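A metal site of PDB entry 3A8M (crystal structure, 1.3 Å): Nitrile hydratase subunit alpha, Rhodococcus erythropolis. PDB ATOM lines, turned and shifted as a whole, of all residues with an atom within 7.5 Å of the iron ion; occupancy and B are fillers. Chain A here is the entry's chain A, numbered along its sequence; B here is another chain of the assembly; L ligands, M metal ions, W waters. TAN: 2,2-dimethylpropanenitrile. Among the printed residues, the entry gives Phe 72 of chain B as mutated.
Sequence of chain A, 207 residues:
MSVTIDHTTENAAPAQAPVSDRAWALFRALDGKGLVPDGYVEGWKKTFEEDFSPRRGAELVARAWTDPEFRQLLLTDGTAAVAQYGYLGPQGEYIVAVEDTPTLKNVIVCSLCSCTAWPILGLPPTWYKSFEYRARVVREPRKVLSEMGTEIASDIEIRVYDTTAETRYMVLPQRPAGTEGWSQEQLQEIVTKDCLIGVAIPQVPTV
OD1 of CSD 115 lies within salt-bridge range of NH2 of Arg 141 of chain B (2.9 Å). OD2 of CSD 115 is in salt-bridge range of the guanidinium group (NH2) of Arg 56 of chain B (2.8 Å). OD2 of CSD 115 is in salt-bridge range of NH2 of Arg 168, at 3.6 Å. The side-chain hydroxyl (OG1) of Thr 116 is in hydrogen-bond range of the backbone carbonyl oxygen (O) of Ser 114, 2.8 Å away. OD2 of CSD 113 is in salt-bridge range of the guanidinium group (NH2) of Arg 141 of chain B. NE of Arg 56 of chain B is in salt-bridge range of OD1 of CSD 113 (2.9 Å). The side-chain sulfur (SG) of Cys 110 lies close to the backbone carbonyl oxygen (O) of Thr 163 (3.4 Å). The backbone NH (N) of Cys 110 is in hydrogen-bond range of the side-chain hydroxyl (OH) of Tyr 128.
Water W1 lies within hydrogen-bond range of the side-chain hydroxyl of Ser 114, OD1 of CSD 113, OD2 of CSD 115 and a nitrogen (N) of the ligand.
The side-chain hydroxyl (OG) of Ser 114 sits at hydrogen-bond distance from a nitrogen (N) of the ligand, at 3.2 Å.
The iron ion is bound by water W1, at 2.0 Å. N of CSD 115 binds the iron ion, 2.0 Å away. N of Ser 114 is bound to the iron ion (2.0 Å). The iron ion is bound by SG of CSD 113. SG of CSD 115 is bound to the iron ion (2.2 Å). SG of Cys 110 binds the iron ion (2.3 Å). The iron ion has six donor atoms within binding distance.
Four residues have an atom within 4 Å of the iron ion: Cys 110, CSD 113, Ser 114 and CSD 115. The nearest printed residue that does not touch the iron ion is Arg 141 of chain B (4.9 Å).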
ATOM      1  N   GLN A  91      20.342 -16.336 -36.790  1.00  0.00           N
ATOM      2  CA  GLN A  91      19.703 -17.238 -35.847  1.00  0.00           C
ATOM      3  C   GLN A  91      18.261 -16.779 -35.569  1.00  0.00           C
ATOM      4  O   GLN A  91      17.711 -17.003 -34.488  1.00  0.00           O
ATOM      5  CB  GLN A  91      20.502 -17.454 -34.551  1.00  0.00           C
ATOM      6  CG  GLN A  91      21.889 -18.082 -34.824  1.00  0.00           C
ATOM      7  CD  GLN A  91      21.696 -19.467 -35.449  1.00  0.00           C
ATOM      8  OE1 GLN A  91      21.028 -20.288 -34.801  1.00  0.00           O
ATOM      9  NE2 GLN A  91      22.214 -19.714 -36.631  1.00  0.00           N
ATOM     10  N   VAL A 109      13.797 -25.211 -25.825  1.00  0.00           N
ATOM     11  CA  VAL A 109      15.151 -25.648 -25.475  1.00  0.00           C
ATOM     12  C   VAL A 109      15.888 -25.921 -26.782  1.00  0.00           C
ATOM     13  O   VAL A 109      15.277 -26.075 -27.860  1.00  0.00           O
ATOM     14  CB  VAL A 109      15.105 -26.899 -24.590  1.00  0.00           C
ATOM     15  CG1 VAL A 109      14.491 -28.059 -25.385  1.00  0.00           C
ATOM     16  CG2 VAL A 109      16.482 -27.291 -24.065  1.00  0.00           C
ATOM     17  N   CYS A 110      17.212 -26.034 -26.722  1.00  0.00           N
ATOM     18  CA  CYS A 110      18.035 -26.666 -27.768  1.00  0.00           C
ATOM     19  C   CYS A 110      18.805 -27.792 -27.060  1.00  0.00           C
ATOM     20  O   CYS A 110      19.891 -27.562 -26.469  1.00  0.00           O
ATOM     21  CB  CYS A 110      18.966 -25.665 -28.420  1.00  0.00           C
ATOM     22  SG  CYS A 110      20.047 -26.459 -29.662  1.00  0.00           S
ATOM     23  N   SER A 111      18.262 -29.011 -27.050  1.00  0.00           N
ATOM     24  CA  SER A 111      18.908 -30.051 -26.259  1.00  0.00           C
ATOM     25  C   SER A 111      20.284 -30.373 -26.833  1.00  0.00           C
ATOM     26  O   SER A 111      21.115 -30.862 -26.072  1.00  0.00           O
ATOM     27  CB  SER A 111      18.064 -31.324 -26.208  1.00  0.00           C
ATOM     28  OG  SER A 111      17.953 -31.958 -27.492  1.00  0.00           O
ATOM     29  N   LEU A 112      20.510 -30.171 -28.128  1.00  0.00           N
ATOM     30  CA  LEU A 112      21.770 -30.549 -28.761  1.00  0.00           C
ATOM     31  C   LEU A 112      22.837 -29.479 -28.629  1.00  0.00           C
ATOM     32  O   LEU A 112      23.998 -29.802 -28.947  1.00  0.00           O
ATOM     33  CB  LEU A 112      21.527 -30.889 -30.248  1.00  0.00           C
ATOM     34  CG  LEU A 112      20.624 -32.096 -30.495  1.00  0.00           C
ATOM     35  CD1 LEU A 112      20.222 -32.193 -31.963  1.00  0.00           C
ATOM     36  CD2 LEU A 112      21.299 -33.397 -30.054  1.00  0.00           C
ATOM     37  N   CSD A 113      22.506 -28.239 -28.201  1.00  0.00           N
ATOM     38  CA  CSD A 113      23.509 -27.149 -28.138  1.00  0.00           C
ATOM     39  CB  CSD A 113      24.136 -26.844 -29.511  1.00  0.00           C
ATOM     40  SG  CSD A 113      23.011 -26.521 -30.876  1.00  0.00           S
ATOM     41  C   CSD A 113      22.874 -25.904 -27.513  1.00  0.00           C
ATOM     42  O   CSD A 113      22.959 -25.837 -26.262  1.00  0.00           O
ATOM     43  OD1 CSD A 113      23.891 -26.095 -31.959  1.00  0.00           O
ATOM     44  OD2 CSD A 113      22.371 -27.842 -31.205  1.00  0.00           O
ATOM     45  N   SER A 114      22.292 -24.966 -28.257  1.00  0.00           N
ATOM     46  CA  SER A 114      21.866 -23.754 -27.501  1.00  0.00           C
ATOM     47  C   SER A 114      20.963 -22.893 -28.386  1.00  0.00           C
ATOM     48  O   SER A 114      20.618 -21.750 -28.006  1.00  0.00           O
ATOM     49  CB  SER A 114      23.064 -22.927 -27.066  1.00  0.00           C
ATOM     50  OG  SER A 114      23.760 -22.473 -28.231  1.00  0.00           O
ATOM     51  N   CSD A 115      20.615 -23.422 -29.553  1.00  0.00           N
ATOM     52  CA  CSD A 115      19.849 -22.661 -30.530  1.00  0.00           C
ATOM     53  CB  CSD A 115      19.384 -23.626 -31.635  1.00  0.00           C
ATOM     54  SG  CSD A 115      20.838 -24.540 -32.122  1.00  0.00           S
ATOM     55  C   CSD A 115      18.649 -21.905 -29.935  1.00  0.00           C
ATOM     56  O   CSD A 115      17.873 -22.457 -29.142  1.00  0.00           O
ATOM     57  OD1 CSD A 115      20.338 -25.643 -32.921  1.00  0.00           O
ATOM     58  OD2 CSD A 115      21.656 -23.573 -32.966  1.00  0.00           O
ATOM     59  N   THR A 116      18.564 -20.648 -30.321  1.00  0.00           N
ATOM     60  CA  THR A 116      17.734 -19.595 -29.766  1.00  0.00           C
ATOM     61  C   THR A 116      17.491 -18.558 -30.850  1.00  0.00           C
ATOM     62  O   THR A 116      18.398 -18.294 -31.637  1.00  0.00           O
ATOM     63  CB  THR A 116      18.520 -18.923 -28.605  1.00  0.00           C
ATOM     64  OG1 THR A 116      18.627 -19.818 -27.498  1.00  0.00           O
ATOM     65  CG2 THR A 116      17.843 -17.665 -28.076  1.00  0.00           C
ATOM     66  N   PRO A 124      21.350 -16.650 -25.727  1.00  0.00           N
ATOM     67  CA  PRO A 124      20.857 -17.411 -24.583  1.00  0.00           C
ATOM     68  C   PRO A 124      21.744 -17.198 -23.359  1.00  0.00           C
ATOM     69  O   PRO A 124      22.945 -17.038 -23.452  1.00  0.00           O
ATOM     70  CB  PRO A 124      20.940 -18.890 -25.012  1.00  0.00           C
ATOM     71  CG  PRO A 124      21.984 -18.848 -26.104  1.00  0.00           C
ATOM     72  CD  PRO A 124      21.810 -17.502 -26.826  1.00  0.00           C
ATOM     73  N   TYR A 128      20.341 -21.635 -19.854  1.00  0.00           N
ATOM     74  CA  TYR A 128      19.624 -22.299 -20.962  1.00  0.00           C
ATOM     75  C   TYR A 128      20.564 -23.237 -21.704  1.00  0.00           C
ATOM     76  O   TYR A 128      20.099 -24.227 -22.290  1.00  0.00           O
ATOM     77  CB  TYR A 128      19.089 -21.233 -21.893  1.00  0.00           C
ATOM     78  CG  TYR A 128      18.436 -21.615 -23.159  1.00  0.00           C
ATOM     79  CD1 TYR A 128      19.118 -21.862 -24.342  1.00  0.00           C
ATOM     80  CD2 TYR A 128      17.033 -21.750 -23.200  1.00  0.00           C
ATOM     81  CE1 TYR A 128      18.510 -22.229 -25.527  1.00  0.00           C
ATOM     82  CE2 TYR A 128      16.401 -22.090 -24.394  1.00  0.00           C
ATOM     83  CZ  TYR A 128      17.131 -22.326 -25.538  1.00  0.00           C
ATOM     84  OH  TYR A 128      16.466 -22.634 -26.713  1.00  0.00           O
ATOM     85  N   LYS A 129      21.863 -22.915 -21.715  1.00  0.00           N
ATOM     86  CA  LYS A 129      22.878 -23.712 -22.380  1.00  0.00           C
ATOM     87  C   LYS A 129      23.424 -24.808 -21.457  1.00  0.00           C
ATOM     88  O   LYS A 129      24.290 -25.584 -21.865  1.00  0.00           O
ATOM     89  CB  LYS A 129      24.068 -22.787 -22.762  1.00  0.00           C
ATOM     90  CG  LYS A 129      23.609 -21.706 -23.721  1.00  0.00           C
ATOM     91  CD  LYS A 129      24.769 -20.772 -24.064  1.00  0.00           C
ATOM     92  CE  LYS A 129      25.196 -19.838 -22.974  1.00  0.00           C
ATOM     93  NZ  LYS A 129      25.922 -18.656 -23.448  1.00  0.00           N
ATOM     94  N   ARG A 134      19.339 -28.746 -20.767  1.00  0.00           N
ATOM     95  CA  ARG A 134      19.337 -29.537 -22.014  1.00  0.00           C
ATOM     96  C   ARG A 134      18.925 -30.986 -21.779  1.00  0.00           C
ATOM     97  O   ARG A 134      18.242 -31.579 -22.629  1.00  0.00           O
ATOM     98  CB  ARG A 134      20.732 -29.476 -22.653  1.00  0.00           C
ATOM     99  CG  ARG A 134      21.051 -28.090 -23.211  1.00  0.00           C
ATOM    100  CD  ARG A 134      22.473 -27.913 -23.736  1.00  0.00           C
ATOM    101  NE  ARG A 134      22.787 -29.051 -24.630  1.00  0.00           N
ATOM    102  CZ  ARG A 134      24.031 -29.453 -24.932  1.00  0.00           C
ATOM    103  NH1 ARG A 134      25.102 -28.799 -24.481  1.00  0.00           N
ATOM    104  NH2 ARG A 134      24.217 -30.528 -25.710  1.00  0.00           N
ATOM    105  N   THR A 163      14.705 -27.177 -30.346  1.00  0.00           N
ATOM    106  CA  THR A 163      15.170 -26.425 -31.500  1.00  0.00           C
ATOM    107  C   THR A 163      16.298 -27.229 -32.166  1.00  0.00           C
ATOM    108  O   THR A 163      17.458 -27.041 -31.795  1.00  0.00           O
ATOM    109  CB  THR A 163      15.674 -25.029 -31.034  1.00  0.00           C
ATOM    110  OG1 THR A 163      14.620 -24.398 -30.285  1.00  0.00           O
ATOM    111  CG2 THR A 163      16.011 -24.173 -32.244  1.00  0.00           C
ATOM    112  N   THR A 164      15.918 -28.097 -33.100  1.00  0.00           N
ATOM    113  CA  THR A 164      16.849 -29.044 -33.712  1.00  0.00           C
ATOM    114  C   THR A 164      17.180 -28.693 -35.156  1.00  0.00           C
ATOM    115  O   THR A 164      18.045 -29.330 -35.750  1.00  0.00           O
ATOM    116  CB  THR A 164      16.231 -30.475 -33.682  1.00  0.00           C
ATOM    117  OG1 THR A 164      14.850 -30.387 -34.119  1.00  0.00           O
ATOM    118  CG2 THR A 164      16.243 -31.020 -32.255  1.00  0.00           C
ATOM    119  N   ARG A 168      13.231 -21.016 -35.450  1.00  0.00           N
ATOM    120  CA  ARG A 168      13.620 -20.342 -34.221  1.00  0.00           C
ATOM    121  C   ARG A 168      12.350 -19.842 -33.550  1.00  0.00           C
ATOM    122  O   ARG A 168      11.518 -19.181 -34.210  1.00  0.00           O
ATOM    123  CB  ARG A 168      14.613 -19.212 -34.506  1.00  0.00           C
ATOM    124  CG  ARG A 168      15.927 -19.749 -35.036  1.00  0.00           C
ATOM    125  CD  ARG A 168      16.816 -20.289 -33.928  1.00  0.00           C
ATOM    126  NE  ARG A 168      18.046 -20.887 -34.477  1.00  0.00           N
ATOM    127  CZ  ARG A 168      18.124 -22.095 -35.031  1.00  0.00           C
ATOM    128  NH1 ARG A 168      17.059 -22.876 -35.124  1.00  0.00           N
ATOM    129  NH2 ARG A 168      19.320 -22.516 -35.517  1.00  0.00           N
ATOM    130  N   ARG B  56      28.632 -26.842 -35.521  1.00  0.00           N
ATOM    131  CA  ARG B  56      27.958 -27.740 -34.568  1.00  0.00           C
ATOM    132  C   ARG B  56      28.695 -29.090 -34.517  1.00  0.00           C
ATOM    133  O   ARG B  56      28.973 -29.620 -33.441  1.00  0.00           O
ATOM    134  CB  ARG B  56      26.509 -27.955 -34.925  1.00  0.00           C
ATOM    135  CG  ARG B  56      25.639 -26.696 -34.950  1.00  0.00           C
ATOM    136  CD  ARG B  56      24.139 -27.123 -34.983  1.00  0.00           C
ATOM    137  NE  ARG B  56      23.349 -25.889 -34.851  1.00  0.00           N
ATOM    138  CZ  ARG B  56      23.011 -25.103 -35.885  1.00  0.00           C
ATOM    139  NH1 ARG B  56      23.330 -25.495 -37.116  1.00  0.00           N
ATOM    140  NH2 ARG B  56      22.353 -23.990 -35.686  1.00  0.00           N
ATOM    141  N   PHE B  72      30.507 -23.438 -22.126  1.00  0.00           N
ATOM    142  CA  PHE B  72      29.922 -23.234 -23.450  1.00  0.00           C
ATOM    143  C   PHE B  72      30.792 -22.455 -24.437  1.00  0.00           C
ATOM    144  O   PHE B  72      31.158 -22.919 -25.515  1.00  0.00           O
ATOM    145  CB  PHE B  72      28.555 -22.547 -23.269  1.00  0.00           C
ATOM    146  CG  PHE B  72      27.853 -22.307 -24.595  1.00  0.00           C
ATOM    147  CD1 PHE B  72      27.064 -23.303 -25.157  1.00  0.00           C
ATOM    148  CD2 PHE B  72      27.983 -21.083 -25.262  1.00  0.00           C
ATOM    149  CE1 PHE B  72      26.448 -23.069 -26.376  1.00  0.00           C
ATOM    150  CE2 PHE B  72      27.415 -20.877 -26.507  1.00  0.00           C
ATOM    151  CZ  PHE B  72      26.625 -21.879 -27.061  1.00  0.00           C
ATOM    152  N   TYR B  76      33.225 -23.369 -28.310  1.00  0.00           N
ATOM    153  CA  TYR B  76      33.220 -22.763 -29.640  1.00  0.00           C
ATOM    154  C   TYR B  76      34.567 -22.130 -29.965  1.00  0.00           C
ATOM    155  O   TYR B  76      34.916 -22.108 -31.161  1.00  0.00           O
ATOM    156  CB  TYR B  76      32.050 -21.712 -29.787  1.00  0.00           C
ATOM    157  CG  TYR B  76      30.776 -22.567 -29.752  1.00  0.00           C
ATOM    158  CD1 TYR B  76      30.191 -23.087 -30.897  1.00  0.00           C
ATOM    159  CD2 TYR B  76      30.233 -22.888 -28.517  1.00  0.00           C
ATOM    160  CE1 TYR B  76      29.032 -23.887 -30.781  1.00  0.00           C
ATOM    161  CE2 TYR B  76      29.130 -23.694 -28.397  1.00  0.00           C
ATOM    162  CZ  TYR B  76      28.513 -24.188 -29.540  1.00  0.00           C
ATOM    163  OH  TYR B  76      27.413 -25.012 -29.383  1.00  0.00           O
ATOM    164  N   ARG B 141      20.840 -34.047 -37.107  1.00  0.00           N
ATOM    165  CA  ARG B 141      20.020 -33.194 -36.272  1.00  0.00           C
ATOM    166  C   ARG B 141      18.768 -33.923 -35.804  1.00  0.00           C
ATOM    167  O   ARG B 141      17.663 -33.390 -35.772  1.00  0.00           O
ATOM    168  CB  ARG B 141      19.656 -31.886 -36.999  1.00  0.00           C
ATOM    169  CG  ARG B 141      20.900 -31.034 -37.240  1.00  0.00           C
ATOM    170  CD  ARG B 141      21.629 -30.725 -35.930  1.00  0.00           C
ATOM    171  NE  ARG B 141      20.816 -29.868 -35.091  1.00  0.00           N
ATOM    172  CZ  ARG B 141      21.251 -29.337 -33.935  1.00  0.00           C
ATOM    173  NH1 ARG B 141      22.432 -29.724 -33.448  1.00  0.00           N
ATOM    174  NH2 ARG B 141      20.467 -28.512 -33.279  1.00  0.00           N
HETATM  175  C   TAN L   1      25.554 -21.407 -31.812  1.00  0.00           C
HETATM  176  N   TAN L   1      25.642 -21.633 -30.689  1.00  0.00           N
HETATM  177  C1  TAN L   1      25.373 -23.127 -33.457  1.00  0.00           C
HETATM  178  C2  TAN L   1      25.793 -21.680 -33.254  1.00  0.00           C
HETATM  179  C3  TAN L   1      27.293 -21.600 -33.502  1.00  0.00           C
HETATM  180  C4  TAN L   1      24.916 -20.742 -34.067  1.00  0.00           C
HETATM  181 FE    FE M   1      21.716 -24.951 -30.169  1.00  0.00          FE
HETATM  182  O   HOH W   1      23.201 -23.719 -30.608  1.00  0.00           O
